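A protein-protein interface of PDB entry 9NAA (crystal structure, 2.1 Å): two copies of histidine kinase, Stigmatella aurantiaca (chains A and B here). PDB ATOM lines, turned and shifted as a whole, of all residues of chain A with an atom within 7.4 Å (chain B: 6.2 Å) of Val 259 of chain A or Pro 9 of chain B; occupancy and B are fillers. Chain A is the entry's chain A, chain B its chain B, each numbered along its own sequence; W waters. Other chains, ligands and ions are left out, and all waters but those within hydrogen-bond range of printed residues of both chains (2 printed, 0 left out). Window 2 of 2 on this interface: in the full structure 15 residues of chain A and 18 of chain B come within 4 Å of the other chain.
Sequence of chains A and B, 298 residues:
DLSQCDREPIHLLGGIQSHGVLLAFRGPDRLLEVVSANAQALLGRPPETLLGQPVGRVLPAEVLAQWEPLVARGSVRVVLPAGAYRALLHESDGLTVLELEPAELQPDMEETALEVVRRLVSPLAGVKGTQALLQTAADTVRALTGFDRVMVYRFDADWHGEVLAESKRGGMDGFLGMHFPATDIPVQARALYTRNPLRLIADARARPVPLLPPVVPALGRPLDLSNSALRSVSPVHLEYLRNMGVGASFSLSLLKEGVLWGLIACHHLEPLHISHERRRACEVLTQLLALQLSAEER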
ATOM      1  N   TRP A 159       7.496   6.737 -26.052  1.00  0.00           N
ATOM      2  CA  TRP A 159       7.822   5.358 -26.417  1.00  0.00           C
ATOM      3  C   TRP A 159       9.334   5.142 -26.559  1.00  0.00           C
ATOM      4  O   TRP A 159       9.796   4.405 -27.440  1.00  0.00           O
ATOM      5  CB  TRP A 159       7.080   4.927 -27.689  1.00  0.00           C
ATOM      6  CG  TRP A 159       5.600   4.724 -27.510  1.00  0.00           C
ATOM      7  CD1 TRP A 159       4.595   5.527 -27.967  1.00  0.00           C
ATOM      8  CD2 TRP A 159       4.965   3.641 -26.817  1.00  0.00           C
ATOM      9  NE1 TRP A 159       3.370   5.003 -27.614  1.00  0.00           N
ATOM     10  CE2 TRP A 159       3.569   3.853 -26.898  1.00  0.00           C
ATOM     11  CE3 TRP A 159       5.443   2.510 -26.135  1.00  0.00           C
ATOM     12  CZ2 TRP A 159       2.642   2.974 -26.328  1.00  0.00           C
ATOM     13  CZ3 TRP A 159       4.517   1.641 -25.565  1.00  0.00           C
ATOM     14  CH2 TRP A 159       3.132   1.879 -25.667  1.00  0.00           C
ATOM     15  N   THR A 194       3.479  -6.358 -28.760  1.00  0.00           N
ATOM     16  CA  THR A 194       2.207  -6.363 -28.044  1.00  0.00           C
ATOM     17  C   THR A 194       1.455  -7.654 -28.312  1.00  0.00           C
ATOM     18  O   THR A 194       0.881  -8.252 -27.399  1.00  0.00           O
ATOM     19  CB  THR A 194       1.383  -5.140 -28.457  1.00  0.00           C
ATOM     20  OG1 THR A 194       2.152  -3.952 -28.226  1.00  0.00           O
ATOM     21  CG2 THR A 194       0.047  -5.049 -27.658  1.00  0.00           C
ATOM     22  N   LEU A 254       6.364  -6.869 -21.612  1.00  0.00           N
ATOM     23  CA  LEU A 254       5.640  -6.518 -20.392  1.00  0.00           C
ATOM     24  C   LEU A 254       4.422  -5.713 -20.802  1.00  0.00           C
ATOM     25  O   LEU A 254       4.557  -4.608 -21.333  1.00  0.00           O
ATOM     26  CB  LEU A 254       6.504  -5.714 -19.428  1.00  0.00           C
ATOM     27  CG  LEU A 254       7.702  -6.474 -18.859  1.00  0.00           C
ATOM     28  CD1 LEU A 254       8.460  -5.576 -17.914  1.00  0.00           C
ATOM     29  CD2 LEU A 254       7.222  -7.715 -18.162  1.00  0.00           C
ATOM     30  N   LEU A 255       3.239  -6.280 -20.590  1.00  0.00           N
ATOM     31  CA  LEU A 255       1.996  -5.581 -20.850  1.00  0.00           C
ATOM     32  C   LEU A 255       1.357  -5.131 -19.541  1.00  0.00           C
ATOM     33  O   LEU A 255       1.499  -5.780 -18.504  1.00  0.00           O
ATOM     34  CB  LEU A 255       1.014  -6.463 -21.615  1.00  0.00           C
ATOM     35  CG  LEU A 255       1.386  -7.047 -22.968  1.00  0.00           C
ATOM     36  CD1 LEU A 255       0.127  -7.601 -23.601  1.00  0.00           C
ATOM     37  CD2 LEU A 255       2.004  -6.004 -23.847  1.00  0.00           C
ATOM     38  N   LYS A 256       0.647  -4.006 -19.602  1.00  0.00           N
ATOM     39  CA  LYS A 256      -0.218  -3.580 -18.511  1.00  0.00           C
ATOM     40  C   LYS A 256      -1.596  -3.319 -19.091  1.00  0.00           C
ATOM     41  O   LYS A 256      -1.747  -2.460 -19.970  1.00  0.00           O
ATOM     42  CB  LYS A 256       0.318  -2.335 -17.805  1.00  0.00           C
ATOM     43  CG  LYS A 256      -0.619  -1.828 -16.705  1.00  0.00           C
ATOM     44  CD  LYS A 256      -0.116  -0.508 -16.166  1.00  0.00           C
ATOM     45  CE  LYS A 256      -1.023   0.047 -15.092  1.00  0.00           C
ATOM     46  NZ  LYS A 256      -0.474   1.322 -14.567  1.00  0.00           N
ATOM     47  N   GLU A 257      -2.581  -4.082 -18.626  1.00  0.00           N
ATOM     48  CA  GLU A 257      -3.944  -3.972 -19.127  1.00  0.00           C
ATOM     49  C   GLU A 257      -3.960  -4.050 -20.654  1.00  0.00           C
ATOM     50  O   GLU A 257      -4.564  -3.227 -21.342  1.00  0.00           O
ATOM     51  CB  GLU A 257      -4.616  -2.689 -18.616  1.00  0.00           C
ATOM     52  CG  GLU A 257      -5.135  -2.803 -17.181  1.00  0.00           C
ATOM     53  CD  GLU A 257      -5.149  -1.474 -16.437  1.00  0.00           C
ATOM     54  OE1 GLU A 257      -4.885  -1.467 -15.204  1.00  0.00           O
ATOM     55  OE2 GLU A 257      -5.440  -0.442 -17.085  1.00  0.00           O
ATOM     56  N   GLY A 258      -3.259  -5.053 -21.183  1.00  0.00           N
ATOM     57  CA  GLY A 258      -3.274  -5.310 -22.605  1.00  0.00           C
ATOM     58  C   GLY A 258      -2.522  -4.314 -23.454  1.00  0.00           C
ATOM     59  O   GLY A 258      -2.566  -4.425 -24.684  1.00  0.00           O
ATOM     60  N   VAL A 259      -1.826  -3.354 -22.853  1.00  0.00           N
ATOM     61  CA  VAL A 259      -1.075  -2.346 -23.584  1.00  0.00           C
ATOM     62  C   VAL A 259       0.415  -2.516 -23.300  1.00  0.00           C
ATOM     63  O   VAL A 259       0.819  -2.828 -22.171  1.00  0.00           O
ATOM     64  CB  VAL A 259      -1.574  -0.935 -23.228  1.00  0.00           C
ATOM     65  CG1 VAL A 259      -0.550   0.127 -23.572  1.00  0.00           C
ATOM     66  CG2 VAL A 259      -2.907  -0.672 -23.965  1.00  0.00           C
ATOM     67  N   LEU A 260       1.234  -2.328 -24.335  1.00  0.00           N
ATOM     68  CA  LEU A 260       2.665  -2.525 -24.179  1.00  0.00           C
ATOM     69  C   LEU A 260       3.229  -1.536 -23.167  1.00  0.00           C
ATOM     70  O   LEU A 260       3.055  -0.321 -23.292  1.00  0.00           O
ATOM     71  CB  LEU A 260       3.376  -2.383 -25.521  1.00  0.00           C
ATOM     72  CG  LEU A 260       4.891  -2.625 -25.445  1.00  0.00           C
ATOM     73  CD1 LEU A 260       5.198  -4.077 -25.060  1.00  0.00           C
ATOM     74  CD2 LEU A 260       5.542  -2.232 -26.785  1.00  0.00           C
ATOM     75  N   TRP A 261       3.902  -2.072 -22.154  1.00  0.00           N
ATOM     76  CA  TRP A 261       4.463  -1.292 -21.058  1.00  0.00           C
ATOM     77  C   TRP A 261       5.984  -1.331 -21.020  1.00  0.00           C
ATOM     78  O   TRP A 261       6.629  -0.321 -20.712  1.00  0.00           O
ATOM     79  CB  TRP A 261       3.878  -1.814 -19.728  1.00  0.00           C
ATOM     80  CG  TRP A 261       4.298  -1.112 -18.455  1.00  0.00           C
ATOM     81  CD1 TRP A 261       3.622  -0.108 -17.809  1.00  0.00           C
ATOM     82  CD2 TRP A 261       5.464  -1.388 -17.651  1.00  0.00           C
ATOM     83  NE1 TRP A 261       4.303   0.263 -16.671  1.00  0.00           N
ATOM     84  CE2 TRP A 261       5.427  -0.510 -16.544  1.00  0.00           C
ATOM     85  CE3 TRP A 261       6.512  -2.308 -17.746  1.00  0.00           C
ATOM     86  CZ2 TRP A 261       6.415  -0.506 -15.550  1.00  0.00           C
ATOM     87  CZ3 TRP A 261       7.510  -2.302 -16.746  1.00  0.00           C
ATOM     88  CH2 TRP A 261       7.450  -1.402 -15.673  1.00  0.00           C
ATOM     89  N   GLY A 262       6.586  -2.456 -21.373  1.00  0.00           N
ATOM     90  CA  GLY A 262       8.020  -2.540 -21.216  1.00  0.00           C
ATOM     91  C   GLY A 262       8.521  -3.806 -21.858  1.00  0.00           C
ATOM     92  O   GLY A 262       7.757  -4.593 -22.419  1.00  0.00           O
ATOM     93  N   ASP B   1       3.635   5.128 -23.576  1.00  0.00           N
ATOM     94  CA  ASP B   1       2.297   5.487 -24.047  1.00  0.00           C
ATOM     95  C   ASP B   1       2.260   6.929 -24.569  1.00  0.00           C
ATOM     96  O   ASP B   1       3.306   7.454 -24.893  1.00  0.00           O
ATOM     97  CB  ASP B   1       1.298   5.284 -22.934  1.00  0.00           C
ATOM     98  CG  ASP B   1       0.987   3.821 -22.695  1.00  0.00           C
ATOM     99  OD1 ASP B   1       0.765   3.089 -23.687  1.00  0.00           O
ATOM    100  OD2 ASP B   1       0.965   3.407 -21.509  1.00  0.00           O
ATOM    101  N   ASP B   6      -4.017   7.787 -24.418  1.00  0.00           N
ATOM    102  CA  ASP B   6      -3.238   7.106 -25.442  1.00  0.00           C
ATOM    103  C   ASP B   6      -2.600   5.804 -24.939  1.00  0.00           C
ATOM    104  O   ASP B   6      -1.784   5.209 -25.652  1.00  0.00           O
ATOM    105  CB  ASP B   6      -2.193   8.058 -26.015  1.00  0.00           C
ATOM    106  CG  ASP B   6      -2.805   9.142 -26.915  1.00  0.00           C
ATOM    107  OD1 ASP B   6      -3.723   8.824 -27.695  1.00  0.00           O
ATOM    108  OD2 ASP B   6      -2.380  10.320 -26.844  1.00  0.00           O
ATOM    109  N   ARG B   7      -2.937   5.368 -23.722  1.00  0.00           N
ATOM    110  CA  ARG B   7      -2.640   4.020 -23.250  1.00  0.00           C
ATOM    111  C   ARG B   7      -3.880   3.135 -23.299  1.00  0.00           C
ATOM    112  O   ARG B   7      -3.852   2.018 -22.778  1.00  0.00           O
ATOM    113  CB  ARG B   7      -2.120   4.060 -21.800  1.00  0.00           C
ATOM    114  CG  ARG B   7      -1.593   5.437 -21.351  1.00  0.00           C
ATOM    115  CD  ARG B   7      -0.990   5.577 -19.933  1.00  0.00           C
ATOM    116  NE  ARG B   7      -0.129   6.760 -19.881  1.00  0.00           N
ATOM    117  CZ  ARG B   7       0.803   6.993 -18.965  1.00  0.00           C
ATOM    118  NH1 ARG B   7       0.965   6.196 -17.923  1.00  0.00           N
ATOM    119  NH2 ARG B   7       1.595   8.054 -19.102  1.00  0.00           N
ATOM    120  N   GLU B   8      -4.950   3.602 -23.943  1.00  0.00           N
ATOM    121  CA  GLU B   8      -6.254   2.944 -23.920  1.00  0.00           C
ATOM    122  C   GLU B   8      -6.244   1.626 -24.690  1.00  0.00           C
ATOM    123  O   GLU B   8      -5.954   1.627 -25.890  1.00  0.00           O
ATOM    124  CB  GLU B   8      -7.289   3.919 -24.501  1.00  0.00           C
ATOM    125  CG  GLU B   8      -8.727   3.572 -24.199  1.00  0.00           C
ATOM    126  CD  GLU B   8      -9.756   4.476 -24.921  1.00  0.00           C
ATOM    127  OE1 GLU B   8      -9.378   5.529 -25.497  1.00  0.00           O
ATOM    128  OE2 GLU B   8     -10.952   4.093 -24.955  1.00  0.00           O
ATOM    129  N   PRO B   9      -6.591   0.487 -24.065  1.00  0.00           N
ATOM    130  CA  PRO B   9      -6.649  -0.795 -24.803  1.00  0.00           C
ATOM    131  C   PRO B   9      -7.911  -0.899 -25.648  1.00  0.00           C
ATOM    132  O   PRO B   9      -8.849  -1.654 -25.326  1.00  0.00           O
ATOM    133  CB  PRO B   9      -6.618  -1.828 -23.672  1.00  0.00           C
ATOM    134  CG  PRO B   9      -7.319  -1.148 -22.539  1.00  0.00           C
ATOM    135  CD  PRO B   9      -7.005   0.330 -22.657  1.00  0.00           C
ATOM    136  N   ILE B  10      -7.920  -0.152 -26.760  1.00  0.00           N
ATOM    137  CA  ILE B  10      -9.137  -0.007 -27.549  1.00  0.00           C
ATOM    138  C   ILE B  10      -9.581  -1.299 -28.192  1.00  0.00           C
ATOM    139  O   ILE B  10     -10.688  -1.359 -28.730  1.00  0.00           O
ATOM    140  CB  ILE B  10      -8.999   1.073 -28.633  1.00  0.00           C
ATOM    141  CG1 ILE B  10      -7.860   0.733 -29.594  1.00  0.00           C
ATOM    142  CG2 ILE B  10      -8.720   2.411 -27.983  1.00  0.00           C
ATOM    143  CD1 ILE B  10      -7.844   1.605 -30.844  1.00  0.00           C
ATOM    144  N   HIS B  11      -8.757  -2.330 -28.151  1.00  0.00           N
ATOM    145  CA  HIS B  11      -9.153  -3.647 -28.627  1.00  0.00           C
ATOM    146  C   HIS B  11      -9.795  -4.478 -27.534  1.00  0.00           C
ATOM    147  O   HIS B  11     -10.238  -5.597 -27.804  1.00  0.00           O
ATOM    148  CB  HIS B  11      -7.927  -4.407 -29.182  1.00  0.00           C
ATOM    149  CG  HIS B  11      -6.810  -4.539 -28.192  1.00  0.00           C
ATOM    150  ND1 HIS B  11      -6.084  -5.700 -28.025  1.00  0.00           N
ATOM    151  CD2 HIS B  11      -6.291  -3.645 -27.317  1.00  0.00           C
ATOM    152  CE1 HIS B  11      -5.166  -5.514 -27.093  1.00  0.00           C
ATOM    153  NE2 HIS B  11      -5.269  -4.274 -26.649  1.00  0.00           N
ATOM    154  N   LEU B  12      -9.839  -3.974 -26.312  1.00  0.00           N
ATOM    155  CA  LEU B  12     -10.324  -4.751 -25.180  1.00  0.00           C
ATOM    156  C   LEU B  12     -11.450  -4.026 -24.454  1.00  0.00           C
ATOM    157  O   LEU B  12     -11.651  -4.255 -23.270  1.00  0.00           O
ATOM    158  CB  LEU B  12      -9.189  -5.075 -24.198  1.00  0.00           C
ATOM    159  CG  LEU B  12      -7.942  -5.826 -24.704  1.00  0.00           C
ATOM    160  CD1 LEU B  12      -6.909  -6.017 -23.577  1.00  0.00           C
ATOM    161  CD2 LEU B  12      -8.271  -7.160 -25.377  1.00  0.00           C
ATOM    162  N   LEU B  13     -12.194  -3.145 -25.138  1.00  0.00           N
ATOM    163  CA  LEU B  13     -13.204  -2.351 -24.430  1.00  0.00           C
ATOM    164  C   LEU B  13     -14.430  -3.166 -24.052  1.00  0.00           C
ATOM    165  O   LEU B  13     -15.171  -2.763 -23.148  1.00  0.00           O
ATOM    166  CB  LEU B  13     -13.627  -1.130 -25.260  1.00  0.00           C
ATOM    167  CG  LEU B  13     -12.500  -0.145 -25.596  1.00  0.00           C
ATOM    168  CD1 LEU B  13     -13.007   1.011 -26.363  1.00  0.00           C
ATOM    169  CD2 LEU B  13     -11.891   0.368 -24.330  1.00  0.00           C
ATOM    170  N   GLN B 188      -2.132   2.387 -30.622  1.00  0.00           N
ATOM    171  CA  GLN B 188      -3.078   1.280 -30.686  1.00  0.00           C
ATOM    172  C   GLN B 188      -4.108   1.512 -31.786  1.00  0.00           C
ATOM    173  O   GLN B 188      -4.527   0.563 -32.460  1.00  0.00           O
ATOM    174  CB  GLN B 188      -3.767   1.132 -29.331  1.00  0.00           C
ATOM    175  CG  GLN B 188      -2.846   0.804 -28.169  1.00  0.00           C
ATOM    176  CD  GLN B 188      -2.232   2.071 -27.558  1.00  0.00           C
ATOM    177  OE1 GLN B 188      -2.741   3.188 -27.749  1.00  0.00           O
ATOM    178  NE2 GLN B 188      -1.147   1.895 -26.796  1.00  0.00           N
HETATM  179  O   HOH W   1      -3.033  -6.692 -25.475  1.00  0.00           O
HETATM  180  O   HOH W   2       3.227   2.374 -21.748  1.00  0.00           O
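A ring nitrogen (NE2) of His 11 of chain B lies within hydrogen-bond range of the backbone carbonyl oxygen (O) of Gly 258 of chain A (3.3 Å).
OD2 of Asp 1 of chain B lies within salt-bridge range of NE of Arg 7 of chain B, at 3.9 Å. The backbone carbonyl oxygen (O) of Asp 6 of chain B sits close to the side-chain amide oxygen (OE1) of Gln 188 of chain B (3.1 Å).
Of chain A, only Glu 257 and Val 259 come within 4 Å of Pro 9 of chain B. Of the printed residues of chain B, Gly 258 of chain A touches His 11 (3.3 Å) and Leu 12 (3.8 Å). Of the printed residues of chain A, His 11 of chain B touches Gly 258 (3.3 Å). Of the printed residues of chain B, Glu 257 of chain A touches Pro 9. Of the printed residues of chain A, Arg 7 of chain B touches Val 259. Printed residues of chain A within 4 Å of Leu 12 of chain B: Gly 258. Leu 260 of chain A touches none of the printed residues of chain B. Lys 256 of chain A touches none of the printed residues of chain B. The nearest residue of chain A that does not touch Pro 9 of chain B is Gly 258 of chain A (4.8 Å). The nearest printed residue of chain A that does not touch Leu 12 of chain B is Glu 257 of chain A (4.3 Å).
Water W1 bridges the backbone carbonyl oxygen (O) of Gly 258 of chain A and a ring nitrogen (NE2) of His 11 of chain B. Water W2 lies within hydrogen-bond range of the side-chain carboxylate of Asp 1 of chain B (2.5 Å) and the backbone carbonyl oxygen of Leu 260 of chain A (3.1 Å).
Of the 11 printed residues of chain A, 4 touch a printed residue of chain B. Hydrophobic or aromatic side chains of chain A that line the printed part of chain B: Trp 159 and Val 259. Hydrophobic or aromatic side chains of chain B that line the printed part of chain A: Pro 9, His 11 and Leu 12. Among the printed residues, 9 pairs touch across the chains. Among the printed residues, no Asp or Glu carboxylate lies within 4 Å of a Lys or Arg side-chain nitrogen of the other chain.
No position is printed for both chains.
Trp 159 of chain A touches Asp 1 of chain B (CZ2 to OD1, 3.2 Å). NE2 of Gln 188 of chain B touches CZ2 of Trp 159 of chain A (3.97 Å). Pro 9 of chain B touches Glu 257 of chain A. CA of Gly 258 of chain A touches CD1 of Leu 12 of chain B, at 3.8 Å. Asp 1 of chain B touches Val 259 of chain A (OD1 to CG1, 3.2 Å). CG2 of Val 259 of chain A touches O of Arg 7 of chain B, at 3.1 Å. Pro 9 of chain B touches Val 259 of chain A (CA to CG2, 3.8 Å). CG1 of Val 259 of chain A touches NE2 of Gln 188 of chain B (3.7 Å).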
